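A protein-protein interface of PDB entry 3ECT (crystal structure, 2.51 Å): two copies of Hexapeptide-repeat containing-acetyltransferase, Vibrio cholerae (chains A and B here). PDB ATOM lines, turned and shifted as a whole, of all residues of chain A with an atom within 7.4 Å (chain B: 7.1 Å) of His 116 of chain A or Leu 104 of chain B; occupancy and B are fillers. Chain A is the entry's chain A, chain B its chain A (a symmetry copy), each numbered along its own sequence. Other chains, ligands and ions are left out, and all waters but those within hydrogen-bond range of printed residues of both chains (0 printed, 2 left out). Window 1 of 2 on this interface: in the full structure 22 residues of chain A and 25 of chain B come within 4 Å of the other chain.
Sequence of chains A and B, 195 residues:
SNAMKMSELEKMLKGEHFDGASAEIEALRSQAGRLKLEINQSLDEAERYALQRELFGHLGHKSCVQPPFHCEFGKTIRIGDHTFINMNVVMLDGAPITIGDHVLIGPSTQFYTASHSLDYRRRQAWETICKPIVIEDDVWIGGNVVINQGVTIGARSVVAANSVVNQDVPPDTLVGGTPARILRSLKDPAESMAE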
ATOM      1  N   LEU A  92      31.462 -13.893 -14.093  1.00  0.00           N
ATOM      2  CA  LEU A  92      30.867 -14.879 -14.990  1.00  0.00           C
ATOM      3  C   LEU A  92      29.742 -14.197 -15.747  1.00  0.00           C
ATOM      4  O   LEU A  92      28.616 -14.052 -15.237  1.00  0.00           O
ATOM      5  CB  LEU A  92      30.350 -16.105 -14.243  1.00  0.00           C
ATOM      6  CG  LEU A  92      31.424 -16.873 -13.492  1.00  0.00           C
ATOM      7  CD1 LEU A  92      30.779 -18.179 -12.944  1.00  0.00           C
ATOM      8  CD2 LEU A  92      32.625 -17.131 -14.409  1.00  0.00           C
ATOM      9  N   ALA A 114      26.092 -17.171 -13.895  1.00  0.00           N
ATOM     10  CA  ALA A 114      25.865 -18.562 -14.213  1.00  0.00           C
ATOM     11  C   ALA A 114      25.413 -19.361 -13.006  1.00  0.00           C
ATOM     12  O   ALA A 114      25.730 -19.030 -11.876  1.00  0.00           O
ATOM     13  CB  ALA A 114      27.136 -19.165 -14.775  1.00  0.00           C
ATOM     14  N   SER A 115      24.643 -20.403 -13.232  1.00  0.00           N
ATOM     15  CA  SER A 115      24.569 -21.415 -12.229  1.00  0.00           C
ATOM     16  C   SER A 115      23.958 -22.650 -12.858  1.00  0.00           C
ATOM     17  O   SER A 115      23.760 -22.690 -14.072  1.00  0.00           O
ATOM     18  CB  SER A 115      23.890 -20.932 -10.938  1.00  0.00           C
ATOM     19  OG  SER A 115      22.556 -21.357 -10.869  1.00  0.00           O
ATOM     20  N   HIS A 116      23.742 -23.671 -12.034  1.00  0.00           N
ATOM     21  CA  HIS A 116      23.366 -24.986 -12.518  1.00  0.00           C
ATOM     22  C   HIS A 116      22.207 -25.533 -11.709  1.00  0.00           C
ATOM     23  O   HIS A 116      21.804 -24.937 -10.679  1.00  0.00           O
ATOM     24  CB  HIS A 116      24.559 -25.935 -12.448  1.00  0.00           C
ATOM     25  CG  HIS A 116      25.759 -25.446 -13.196  1.00  0.00           C
ATOM     26  ND1 HIS A 116      26.799 -24.763 -12.590  1.00  0.00           N
ATOM     27  CD2 HIS A 116      26.090 -25.542 -14.505  1.00  0.00           C
ATOM     28  CE1 HIS A 116      27.709 -24.450 -13.495  1.00  0.00           C
ATOM     29  NE2 HIS A 116      27.301 -24.912 -14.666  1.00  0.00           N
ATOM     30  N   SER A 117      21.663 -26.642 -12.212  1.00  0.00           N
ATOM     31  CA  SER A 117      20.612 -27.407 -11.552  1.00  0.00           C
ATOM     32  C   SER A 117      21.185 -28.247 -10.406  1.00  0.00           C
ATOM     33  O   SER A 117      22.300 -28.800 -10.508  1.00  0.00           O
ATOM     34  CB  SER A 117      19.955 -28.355 -12.567  1.00  0.00           C
ATOM     35  OG  SER A 117      18.938 -29.166 -11.979  1.00  0.00           O
ATOM     36  N   LEU A 118      20.406 -28.364  -9.330  1.00  0.00           N
ATOM     37  CA  LEU A 118      20.750 -29.256  -8.218  1.00  0.00           C
ATOM     38  C   LEU A 118      20.990 -30.662  -8.663  1.00  0.00           C
ATOM     39  O   LEU A 118      21.921 -31.314  -8.149  1.00  0.00           O
ATOM     40  CB  LEU A 118      19.616 -29.379  -7.229  1.00  0.00           C
ATOM     41  CG  LEU A 118      19.133 -28.192  -6.438  1.00  0.00           C
ATOM     42  CD1 LEU A 118      18.216 -28.861  -5.391  1.00  0.00           C
ATOM     43  CD2 LEU A 118      20.296 -27.389  -5.828  1.00  0.00           C
ATOM     44  N   ASP A 119      20.126 -31.154  -9.559  1.00  0.00           N
ATOM     45  CA  ASP A 119      20.204 -32.523  -9.968  1.00  0.00           C
ATOM     46  C   ASP A 119      21.409 -32.789 -10.856  1.00  0.00           C
ATOM     47  O   ASP A 119      21.633 -32.090 -11.847  1.00  0.00           O
ATOM     48  CB  ASP A 119      18.949 -33.008 -10.628  1.00  0.00           C
ATOM     49  CG  ASP A 119      19.116 -34.421 -11.126  1.00  0.00           C
ATOM     50  OD1 ASP A 119      18.993 -35.395 -10.312  1.00  0.00           O
ATOM     51  OD2 ASP A 119      19.460 -34.546 -12.330  1.00  0.00           O
ATOM     52  N   TYR A 120      22.160 -33.830 -10.497  1.00  0.00           N
ATOM     53  CA  TYR A 120      23.474 -34.086 -11.056  1.00  0.00           C
ATOM     54  C   TYR A 120      23.345 -34.576 -12.501  1.00  0.00           C
ATOM     55  O   TYR A 120      24.282 -34.420 -13.297  1.00  0.00           O
ATOM     56  CB  TYR A 120      24.270 -35.069 -10.155  1.00  0.00           C
ATOM     57  CG  TYR A 120      23.831 -36.528 -10.293  1.00  0.00           C
ATOM     58  CD1 TYR A 120      22.723 -37.026  -9.588  1.00  0.00           C
ATOM     59  CD2 TYR A 120      24.505 -37.393 -11.142  1.00  0.00           C
ATOM     60  CE1 TYR A 120      22.290 -38.321  -9.735  1.00  0.00           C
ATOM     61  CE2 TYR A 120      24.099 -38.707 -11.286  1.00  0.00           C
ATOM     62  CZ  TYR A 120      22.982 -39.167 -10.585  1.00  0.00           C
ATOM     63  OH  TYR A 120      22.609 -40.488 -10.715  1.00  0.00           O
ATOM     64  N   ARG A 122      21.117 -33.401 -14.527  1.00  0.00           N
ATOM     65  CA  ARG A 122      20.846 -32.175 -15.223  1.00  0.00           C
ATOM     66  C   ARG A 122      22.151 -31.368 -15.329  1.00  0.00           C
ATOM     67  O   ARG A 122      22.095 -30.187 -15.647  1.00  0.00           O
ATOM     68  CB  ARG A 122      19.768 -31.390 -14.443  1.00  0.00           C
ATOM     69  CG  ARG A 122      18.548 -30.869 -15.238  1.00  0.00           C
ATOM     70  CD  ARG A 122      17.479 -31.916 -15.535  1.00  0.00           C
ATOM     71  NE  ARG A 122      17.886 -32.740 -16.683  1.00  0.00           N
ATOM     72  CZ  ARG A 122      17.965 -34.073 -16.698  1.00  0.00           C
ATOM     73  NH1 ARG A 122      18.381 -34.690 -17.794  1.00  0.00           N
ATOM     74  NH2 ARG A 122      17.612 -34.804 -15.638  1.00  0.00           N
ATOM     75  N   ARG A 123      23.314 -31.975 -15.040  1.00  0.00           N
ATOM     76  CA  ARG A 123      24.591 -31.219 -15.017  1.00  0.00           C
ATOM     77  C   ARG A 123      25.741 -31.842 -15.822  1.00  0.00           C
ATOM     78  O   ARG A 123      26.812 -31.224 -15.986  1.00  0.00           O
ATOM     79  CB  ARG A 123      25.068 -30.956 -13.585  1.00  0.00           C
ATOM     80  CG  ARG A 123      24.288 -29.898 -12.795  1.00  0.00           C
ATOM     81  CD  ARG A 123      25.110 -29.418 -11.566  1.00  0.00           C
ATOM     82  NE  ARG A 123      25.731 -30.534 -10.830  1.00  0.00           N
ATOM     83  CZ  ARG A 123      25.213 -31.115  -9.747  1.00  0.00           C
ATOM     84  NH1 ARG A 123      25.830 -32.116  -9.180  1.00  0.00           N
ATOM     85  NH2 ARG A 123      24.075 -30.693  -9.223  1.00  0.00           N
ATOM     86  N   GLN A 124      25.492 -33.043 -16.347  1.00  0.00           N
ATOM     87  CA  GLN A 124      26.513 -33.856 -17.002  1.00  0.00           C
ATOM     88  C   GLN A 124      27.045 -33.272 -18.303  1.00  0.00           C
ATOM     89  O   GLN A 124      28.204 -33.548 -18.702  1.00  0.00           O
ATOM     90  CB  GLN A 124      25.963 -35.227 -17.229  1.00  0.00           C
ATOM     91  CG  GLN A 124      25.394 -35.816 -15.967  1.00  0.00           C
ATOM     92  CD  GLN A 124      26.103 -37.063 -15.535  1.00  0.00           C
ATOM     93  OE1 GLN A 124      26.760 -37.734 -16.334  1.00  0.00           O
ATOM     94  NE2 GLN A 124      25.944 -37.415 -14.274  1.00  0.00           N
ATOM     95  N   ALA A 125      26.211 -32.433 -18.923  1.00  0.00           N
ATOM     96  CA  ALA A 125      26.580 -31.693 -20.118  1.00  0.00           C
ATOM     97  C   ALA A 125      27.031 -30.254 -19.802  1.00  0.00           C
ATOM     98  O   ALA A 125      27.283 -29.463 -20.716  1.00  0.00           O
ATOM     99  CB  ALA A 125      25.416 -31.702 -21.125  1.00  0.00           C
ATOM    100  N   TRP A 126      27.168 -29.944 -18.510  1.00  0.00           N
ATOM    101  CA  TRP A 126      27.587 -28.634 -18.025  1.00  0.00           C
ATOM    102  C   TRP A 126      26.582 -27.562 -18.421  1.00  0.00           C
ATOM    103  O   TRP A 126      26.948 -26.416 -18.714  1.00  0.00           O
ATOM    104  CB  TRP A 126      28.989 -28.263 -18.527  1.00  0.00           C
ATOM    105  CG  TRP A 126      30.044 -29.305 -18.296  1.00  0.00           C
ATOM    106  CD1 TRP A 126      29.929 -30.444 -17.546  1.00  0.00           C
ATOM    107  CD2 TRP A 126      31.394 -29.283 -18.780  1.00  0.00           C
ATOM    108  NE1 TRP A 126      31.118 -31.143 -17.542  1.00  0.00           N
ATOM    109  CE2 TRP A 126      32.037 -30.460 -18.292  1.00  0.00           C
ATOM    110  CE3 TRP A 126      32.127 -28.394 -19.580  1.00  0.00           C
ATOM    111  CZ2 TRP A 126      33.377 -30.765 -18.577  1.00  0.00           C
ATOM    112  CZ3 TRP A 126      33.479 -28.705 -19.863  1.00  0.00           C
ATOM    113  CH2 TRP A 126      34.073 -29.883 -19.367  1.00  0.00           C
ATOM    114  N   GLU A 127      25.308 -27.923 -18.440  1.00  0.00           N
ATOM    115  CA  GLU A 127      24.303 -26.937 -18.782  1.00  0.00           C
ATOM    116  C   GLU A 127      24.294 -25.869 -17.705  1.00  0.00           C
ATOM    117  O   GLU A 127      24.234 -26.174 -16.516  1.00  0.00           O
ATOM    118  CB  GLU A 127      22.914 -27.555 -19.018  1.00  0.00           C
ATOM    119  CG  GLU A 127      22.582 -28.807 -18.203  1.00  0.00           C
ATOM    120  CD  GLU A 127      23.188 -30.124 -18.753  1.00  0.00           C
ATOM    121  OE1 GLU A 127      22.580 -30.725 -19.675  1.00  0.00           O
ATOM    122  OE2 GLU A 127      24.233 -30.579 -18.220  1.00  0.00           O
ATOM    123  N   THR A 128      24.425 -24.623 -18.163  1.00  0.00           N
ATOM    124  CA  THR A 128      24.484 -23.415 -17.330  1.00  0.00           C
ATOM    125  C   THR A 128      23.173 -22.680 -17.517  1.00  0.00           C
ATOM    126  O   THR A 128      22.699 -22.554 -18.634  1.00  0.00           O
ATOM    127  CB  THR A 128      25.616 -22.484 -17.838  1.00  0.00           C
ATOM    128  OG1 THR A 128      26.812 -23.246 -17.997  1.00  0.00           O
ATOM    129  CG2 THR A 128      25.903 -21.419 -16.884  1.00  0.00           C
ATOM    130  N   ILE A 129      22.561 -22.209 -16.446  1.00  0.00           N
ATOM    131  CA  ILE A 129      21.610 -21.145 -16.685  1.00  0.00           C
ATOM    132  C   ILE A 129      22.114 -19.806 -16.171  1.00  0.00           C
ATOM    133  O   ILE A 129      22.802 -19.733 -15.159  1.00  0.00           O
ATOM    134  CB  ILE A 129      20.175 -21.470 -16.264  1.00  0.00           C
ATOM    135  CG1 ILE A 129      19.232 -21.100 -17.409  1.00  0.00           C
ATOM    136  CG2 ILE A 129      19.778 -20.773 -14.935  1.00  0.00           C
ATOM    137  CD1 ILE A 129      18.219 -22.242 -17.771  1.00  0.00           C
ATOM    138  N   CYS A 130      21.765 -18.770 -16.913  1.00  0.00           N
ATOM    139  CA  CYS A 130      22.268 -17.453 -16.710  1.00  0.00           C
ATOM    140  C   CYS A 130      21.128 -16.468 -16.531  1.00  0.00           C
ATOM    141  O   CYS A 130      20.130 -16.493 -17.275  1.00  0.00           O
ATOM    142  CB  CYS A 130      23.121 -17.046 -17.899  1.00  0.00           C
ATOM    143  SG  CYS A 130      24.620 -18.021 -17.965  1.00  0.00           S
ATOM    144  N   GLN A 149      23.220 -14.676  -9.524  1.00  0.00           N
ATOM    145  CA  GLN A 149      22.311 -14.388 -10.635  1.00  0.00           C
ATOM    146  C   GLN A 149      21.069 -13.610 -10.282  1.00  0.00           C
ATOM    147  O   GLN A 149      20.460 -13.830  -9.242  1.00  0.00           O
ATOM    148  CB  GLN A 149      21.645 -15.681 -11.100  1.00  0.00           C
ATOM    149  CG  GLN A 149      22.451 -16.794 -11.497  1.00  0.00           C
ATOM    150  CD  GLN A 149      21.570 -17.870 -12.146  1.00  0.00           C
ATOM    151  OE1 GLN A 149      20.685 -18.458 -11.515  1.00  0.00           O
ATOM    152  NE2 GLN A 149      21.816 -18.115 -13.416  1.00  0.00           N
ATOM    153  N   HIS B  82      35.299 -35.274 -17.968  1.00  0.00           N
ATOM    154  CA  HIS B  82      34.202 -34.312 -18.078  1.00  0.00           C
ATOM    155  C   HIS B  82      34.036 -33.472 -16.826  1.00  0.00           C
ATOM    156  O   HIS B  82      32.914 -33.189 -16.394  1.00  0.00           O
ATOM    157  CB  HIS B  82      32.862 -34.997 -18.364  1.00  0.00           C
ATOM    158  CG  HIS B  82      32.924 -36.042 -19.431  1.00  0.00           C
ATOM    159  ND1 HIS B  82      32.754 -35.751 -20.770  1.00  0.00           N
ATOM    160  CD2 HIS B  82      33.099 -37.385 -19.352  1.00  0.00           C
ATOM    161  CE1 HIS B  82      32.843 -36.868 -21.473  1.00  0.00           C
ATOM    162  NE2 HIS B  82      33.045 -37.873 -20.635  1.00  0.00           N
ATOM    163  N   THR B  83      35.133 -33.068 -16.214  1.00  0.00           N
ATOM    164  CA  THR B  83      34.958 -32.146 -15.129  1.00  0.00           C
ATOM    165  C   THR B  83      35.423 -30.776 -15.570  1.00  0.00           C
ATOM    166  O   THR B  83      36.325 -30.625 -16.429  1.00  0.00           O
ATOM    167  CB  THR B  83      35.532 -32.639 -13.790  1.00  0.00           C
ATOM    168  OG1 THR B  83      36.920 -32.350 -13.687  1.00  0.00           O
ATOM    169  CG2 THR B  83      35.345 -34.059 -13.642  1.00  0.00           C
ATOM    170  N   PHE B  84      34.757 -29.761 -15.051  1.00  0.00           N
ATOM    171  CA  PHE B  84      35.098 -28.422 -15.456  1.00  0.00           C
ATOM    172  C   PHE B  84      35.522 -27.631 -14.225  1.00  0.00           C
ATOM    173  O   PHE B  84      34.812 -27.606 -13.225  1.00  0.00           O
ATOM    174  CB  PHE B  84      33.904 -27.801 -16.155  1.00  0.00           C
ATOM    175  CG  PHE B  84      34.049 -26.331 -16.389  1.00  0.00           C
ATOM    176  CD1 PHE B  84      33.553 -25.409 -15.461  1.00  0.00           C
ATOM    177  CD2 PHE B  84      34.694 -25.863 -17.530  1.00  0.00           C
ATOM    178  CE1 PHE B  84      33.674 -24.020 -15.667  1.00  0.00           C
ATOM    179  CE2 PHE B  84      34.843 -24.476 -17.755  1.00  0.00           C
ATOM    180  CZ  PHE B  84      34.317 -23.545 -16.816  1.00  0.00           C
ATOM    181  N   ILE B  85      36.672 -26.990 -14.284  1.00  0.00           N
ATOM    182  CA  ILE B  85      37.106 -26.121 -13.199  1.00  0.00           C
ATOM    183  C   ILE B  85      37.173 -24.694 -13.713  1.00  0.00           C
ATOM    184  O   ILE B  85      37.932 -24.412 -14.633  1.00  0.00           O
ATOM    185  CB  ILE B  85      38.484 -26.526 -12.641  1.00  0.00           C
ATOM    186  CG1 ILE B  85      38.435 -27.968 -12.127  1.00  0.00           C
ATOM    187  CG2 ILE B  85      38.886 -25.581 -11.499  1.00  0.00           C
ATOM    188  CD1 ILE B  85      39.742 -28.520 -11.632  1.00  0.00           C
ATOM    189  N   ASN B  86      36.384 -23.802 -13.124  1.00  0.00           N
ATOM    190  CA  ASN B  86      36.363 -22.423 -13.570  1.00  0.00           C
ATOM    191  C   ASN B  86      37.600 -21.625 -13.154  1.00  0.00           C
ATOM    192  O   ASN B  86      38.470 -22.145 -12.473  1.00  0.00           O
ATOM    193  CB  ASN B  86      35.116 -21.750 -13.070  1.00  0.00           C
ATOM    194  CG  ASN B  86      34.460 -20.857 -14.129  1.00  0.00           C
ATOM    195  OD1 ASN B  86      33.228 -20.753 -14.163  1.00  0.00           O
ATOM    196  ND2 ASN B  86      35.269 -20.194 -14.972  1.00  0.00           N
ATOM    197  N   ILE B  99      40.018 -35.356  -7.608  1.00  0.00           N
ATOM    198  CA  ILE B  99      38.732 -34.885  -8.161  1.00  0.00           C
ATOM    199  C   ILE B  99      38.181 -35.839  -9.238  1.00  0.00           C
ATOM    200  O   ILE B  99      38.853 -36.115 -10.245  1.00  0.00           O
ATOM    201  CB  ILE B  99      38.895 -33.479  -8.750  1.00  0.00           C
ATOM    202  CG1 ILE B  99      39.520 -32.536  -7.689  1.00  0.00           C
ATOM    203  CG2 ILE B  99      37.548 -32.968  -9.310  1.00  0.00           C
ATOM    204  CD1 ILE B  99      40.106 -31.251  -8.250  1.00  0.00           C
ATOM    205  N   ASP B 101      34.790 -37.563 -11.747  1.00  0.00           N
ATOM    206  CA  ASP B 101      34.207 -37.288 -13.071  1.00  0.00           C
ATOM    207  C   ASP B 101      32.955 -36.447 -12.960  1.00  0.00           C
ATOM    208  O   ASP B 101      32.262 -36.483 -11.945  1.00  0.00           O
ATOM    209  CB  ASP B 101      33.846 -38.590 -13.841  1.00  0.00           C
ATOM    210  CG  ASP B 101      34.929 -39.645 -13.774  1.00  0.00           C
ATOM    211  OD1 ASP B 101      36.121 -39.264 -13.856  1.00  0.00           O
ATOM    212  OD2 ASP B 101      34.591 -40.855 -13.653  1.00  0.00           O
ATOM    213  N   HIS B 102      32.649 -35.717 -14.027  1.00  0.00           N
ATOM    214  CA  HIS B 102      31.497 -34.809 -14.035  1.00  0.00           C
ATOM    215  C   HIS B 102      31.436 -33.813 -12.852  1.00  0.00           C
ATOM    216  O   HIS B 102      30.351 -33.454 -12.367  1.00  0.00           O
ATOM    217  CB  HIS B 102      30.203 -35.604 -14.118  1.00  0.00           C
ATOM    218  CG  HIS B 102      30.026 -36.329 -15.409  1.00  0.00           C
ATOM    219  ND1 HIS B 102      30.185 -37.697 -15.518  1.00  0.00           N
ATOM    220  CD2 HIS B 102      29.685 -35.883 -16.639  1.00  0.00           C
ATOM    221  CE1 HIS B 102      29.948 -38.068 -16.764  1.00  0.00           C
ATOM    222  NE2 HIS B 102      29.645 -36.987 -17.466  1.00  0.00           N
ATOM    223  N   VAL B 103      32.599 -33.361 -12.398  1.00  0.00           N
ATOM    224  CA  VAL B 103      32.642 -32.409 -11.318  1.00  0.00           C
ATOM    225  C   VAL B 103      32.621 -30.972 -11.889  1.00  0.00           C
ATOM    226  O   VAL B 103      33.265 -30.668 -12.908  1.00  0.00           O
ATOM    227  CB  VAL B 103      33.862 -32.669 -10.434  1.00  0.00           C
ATOM    228  CG1 VAL B 103      34.037 -31.563  -9.410  1.00  0.00           C
ATOM    229  CG2 VAL B 103      33.739 -34.034  -9.774  1.00  0.00           C
ATOM    230  N   LEU B 104      31.871 -30.089 -11.250  1.00  0.00           N
ATOM    231  CA  LEU B 104      31.927 -28.681 -11.630  1.00  0.00           C
ATOM    232  C   LEU B 104      32.445 -27.890 -10.465  1.00  0.00           C
ATOM    233  O   LEU B 104      31.866 -27.954  -9.390  1.00  0.00           O
ATOM    234  CB  LEU B 104      30.523 -28.141 -11.984  1.00  0.00           C
ATOM    235  CG  LEU B 104      29.891 -28.632 -13.267  1.00  0.00           C
ATOM    236  CD1 LEU B 104      28.403 -28.332 -13.313  1.00  0.00           C
ATOM    237  CD2 LEU B 104      30.611 -27.986 -14.425  1.00  0.00           C
ATOM    238  N   ILE B 105      33.494 -27.106 -10.700  1.00  0.00           N
ATOM    239  CA  ILE B 105      34.064 -26.258  -9.654  1.00  0.00           C
ATOM    240  C   ILE B 105      33.994 -24.790 -10.069  1.00  0.00           C
ATOM    241  O   ILE B 105      34.552 -24.409 -11.106  1.00  0.00           O
ATOM    242  CB  ILE B 105      35.509 -26.692  -9.299  1.00  0.00           C
ATOM    243  CG1 ILE B 105      35.461 -28.015  -8.558  1.00  0.00           C
ATOM    244  CG2 ILE B 105      36.157 -25.698  -8.377  1.00  0.00           C
ATOM    245  CD1 ILE B 105      36.650 -28.915  -8.785  1.00  0.00           C
ATOM    246  N   GLY B 106      33.319 -23.970  -9.264  1.00  0.00           N
ATOM    247  CA  GLY B 106      33.113 -22.571  -9.602  1.00  0.00           C
ATOM    248  C   GLY B 106      34.367 -21.749  -9.372  1.00  0.00           C
ATOM    249  O   GLY B 106      35.302 -22.194  -8.703  1.00  0.00           O
ATOM    250  N   ILE B 135      37.212 -35.064  -4.006  1.00  0.00           N
ATOM    251  CA  ILE B 135      35.898 -34.689  -4.490  1.00  0.00           C
ATOM    252  C   ILE B 135      35.397 -35.794  -5.387  1.00  0.00           C
ATOM    253  O   ILE B 135      35.979 -36.088  -6.451  1.00  0.00           O
ATOM    254  CB  ILE B 135      35.913 -33.288  -5.153  1.00  0.00           C
ATOM    255  CG1 ILE B 135      36.185 -32.225  -4.094  1.00  0.00           C
ATOM    256  CG2 ILE B 135      34.567 -32.921  -5.853  1.00  0.00           C
ATOM    257  CD1 ILE B 135      37.092 -31.283  -4.652  1.00  0.00           C
ATOM    258  N   ASP B 138      30.384 -36.260  -9.903  1.00  0.00           N
ATOM    259  CA  ASP B 138      29.089 -35.603 -10.073  1.00  0.00           C
ATOM    260  C   ASP B 138      28.782 -34.562  -9.013  1.00  0.00           C
ATOM    261  O   ASP B 138      27.616 -34.266  -8.699  1.00  0.00           O
ATOM    262  CB  ASP B 138      27.965 -36.642 -10.131  1.00  0.00           C
ATOM    263  CG  ASP B 138      27.955 -37.403 -11.440  1.00  0.00           C
ATOM    264  OD1 ASP B 138      27.783 -36.725 -12.495  1.00  0.00           O
ATOM    265  OD2 ASP B 138      28.127 -38.666 -11.403  1.00  0.00           O
ATOM    266  N   VAL B 139      29.845 -33.999  -8.473  1.00  0.00           N
ATOM    267  CA  VAL B 139      29.731 -33.010  -7.431  1.00  0.00           C
ATOM    268  C   VAL B 139      29.732 -31.635  -8.064  1.00  0.00           C
ATOM    269  O   VAL B 139      30.482 -31.362  -9.021  1.00  0.00           O
ATOM    270  CB  VAL B 139      30.888 -33.174  -6.412  1.00  0.00           C
ATOM    271  CG1 VAL B 139      31.112 -31.880  -5.608  1.00  0.00           C
ATOM    272  CG2 VAL B 139      30.595 -34.335  -5.513  1.00  0.00           C
ATOM    273  N   TRP B 140      28.913 -30.744  -7.538  1.00  0.00           N
ATOM    274  CA  TRP B 140      29.004 -29.358  -7.963  1.00  0.00           C
ATOM    275  C   TRP B 140      29.465 -28.463  -6.830  1.00  0.00           C
ATOM    276  O   TRP B 140      28.770 -28.305  -5.822  1.00  0.00           O
ATOM    277  CB  TRP B 140      27.652 -28.877  -8.461  1.00  0.00           C
ATOM    278  CG  TRP B 140      27.567 -27.404  -8.635  1.00  0.00           C
ATOM    279  CD1 TRP B 140      28.604 -26.521  -8.855  1.00  0.00           C
ATOM    280  CD2 TRP B 140      26.354 -26.616  -8.654  1.00  0.00           C
ATOM    281  NE1 TRP B 140      28.099 -25.225  -8.988  1.00  0.00           N
ATOM    282  CE2 TRP B 140      26.730 -25.260  -8.887  1.00  0.00           C
ATOM    283  CE3 TRP B 140      24.984 -26.928  -8.494  1.00  0.00           C
ATOM    284  CZ2 TRP B 140      25.795 -24.221  -8.944  1.00  0.00           C
ATOM    285  CZ3 TRP B 140      24.035 -25.867  -8.564  1.00  0.00           C
ATOM    286  CH2 TRP B 140      24.462 -24.536  -8.766  1.00  0.00           C
ATOM    287  N   ILE B 141      30.638 -27.881  -7.002  1.00  0.00           N
ATOM    288  CA  ILE B 141      31.151 -26.945  -6.040  1.00  0.00           C
ATOM    289  C   ILE B 141      30.987 -25.486  -6.480  1.00  0.00           C
ATOM    290  O   ILE B 141      31.389 -25.104  -7.598  1.00  0.00           O
ATOM    291  CB  ILE B 141      32.556 -27.273  -5.697  1.00  0.00           C
ATOM    292  CG1 ILE B 141      32.523 -28.486  -4.777  1.00  0.00           C
ATOM    293  CG2 ILE B 141      33.164 -26.141  -4.869  1.00  0.00           C
ATOM    294  CD1 ILE B 141      33.796 -29.184  -4.729  1.00  0.00           C
ATOM    295  N   GLY B 142      30.338 -24.686  -5.625  1.00  0.00           N
ATOM    296  CA  GLY B 142      29.921 -23.312  -6.012  1.00  0.00           C
ATOM    297  C   GLY B 142      31.136 -22.429  -6.075  1.00  0.00           C
ATOM    298  O   GLY B 142      32.218 -22.838  -5.606  1.00  0.00           O
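Hydrophobic or aromatic side chains of chain A that line the printed part of chain B: Leu 92, His 116, Tyr 120 and Trp 126.
Along chain A the printed residues that touch a printed residue of chain B span positions 92 to 126.
Printed residues of chain B that touch a printed residue of chain A: His 82, Thr 83, Phe 84, Asn 86, His 102, Leu 104, Asp 138 and Trp 140.
Hydrophobic or aromatic side chains of chain B within 4 Å of the printed part of chain A: Phe 84, His 102, Leu 104 and Trp 140.
Along chain B the printed residues that touch a printed residue of chain A span positions 82 to 140.
Among the printed residues, no Asp or Glu carboxylate lies within 4 Å of a Lys or Arg side-chain nitrogen of the other chain.
The guanidinium group of Arg 123 of chain A is in hydrogen-bond range of the backbone carbonyl oxygen of Asp 138 of chain B (2.8 Å).
NE2 of His 102 of chain B is in hydrogen-bond range of OE1 of Gln 124 of chain A (3.2 Å).
NE2 of Gln 124 of chain A is in hydrogen-bond range of OD1 of Asp 138 of chain B (2.7 Å).
The backbone carbonyl oxygen of His 82 of chain B lies within hydrogen-bond range of the indole nitrogen of Trp 126 of chain A, 3.0 Å away.
Asn 86 of chain B touches Leu 92 of chain A (OD1 to CD2, 3.7 Å).
Leu 104 of chain B touches His 116 of chain A (CD1 to CD2, 3.8 Å).
His 116 of chain A touches Trp 140 of chain B.
Trp 140 of chain B touches Ser 117 of chain A (CE3 to O, 3.8 Å).
Asp 138 of chain B touches Tyr 120 of chain A.
CD of Arg 123 of chain A touches CD1 of Leu 104 of chain B (3.9 Å).
CB of Trp 140 of chain B touches NE of Arg 123 of chain A, at 3.5 Å.
Thr 83 of chain B touches Trp 126 of chain A (C to CZ2, 3.6 Å).
Phe 84 of chain B touches Trp 126 of chain A (CB to CH2, 3.8 Å).
Of the printed residues of chain B, Leu 92 of chain A touches Asn 86 (3.7 Å).
His 116 of chain A touches just these residues of chain B: Leu 104 (3.8 Å) and Trp 140 (3.2 Å).
Printed residues of chain B within 4 Å of Tyr 120 of chain A: Asp 138 (3.5 Å).
Of the printed residues of chain B, Arg 123 of chain A touches Leu 104 (3.9 Å), Asp 138 (2.8 Å) and Trp 140 (3.5 Å).
Of the printed residues of chain A, Leu 104 of chain B touches His 116 (3.8 Å) and Arg 123 (3.9 Å).
No position is printed for both chains.
The side-chain hydroxyl (OG) of Ser 117 of chain A lies close to the backbone NH (N) of Asp 119 of chain A, 3.3 Å away.
The guanidinium group (NH2) of Arg 123 of chain A lies within hydrogen-bond range of the backbone carbonyl oxygen (O) of Ser 117 of chain A, at 2.9 Å.
O of Leu 118 of chain A lies within hydrogen-bond range of NH2 of Arg 123 of chain A (2.5 Å).
The backbone NH (N) of His 102 of chain B sits close to the backbone carbonyl oxygen (O) of His 82 of chain B, at 3.5 Å.
The backbone NH (N) of Ile 105 of chain B lies within hydrogen-bond range of the backbone carbonyl oxygen (O) of Phe 84 of chain B (2.9 Å).
O of Asp 101 of chain B sits at hydrogen-bond distance from N of Asp 138 of chain B (2.8 Å).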
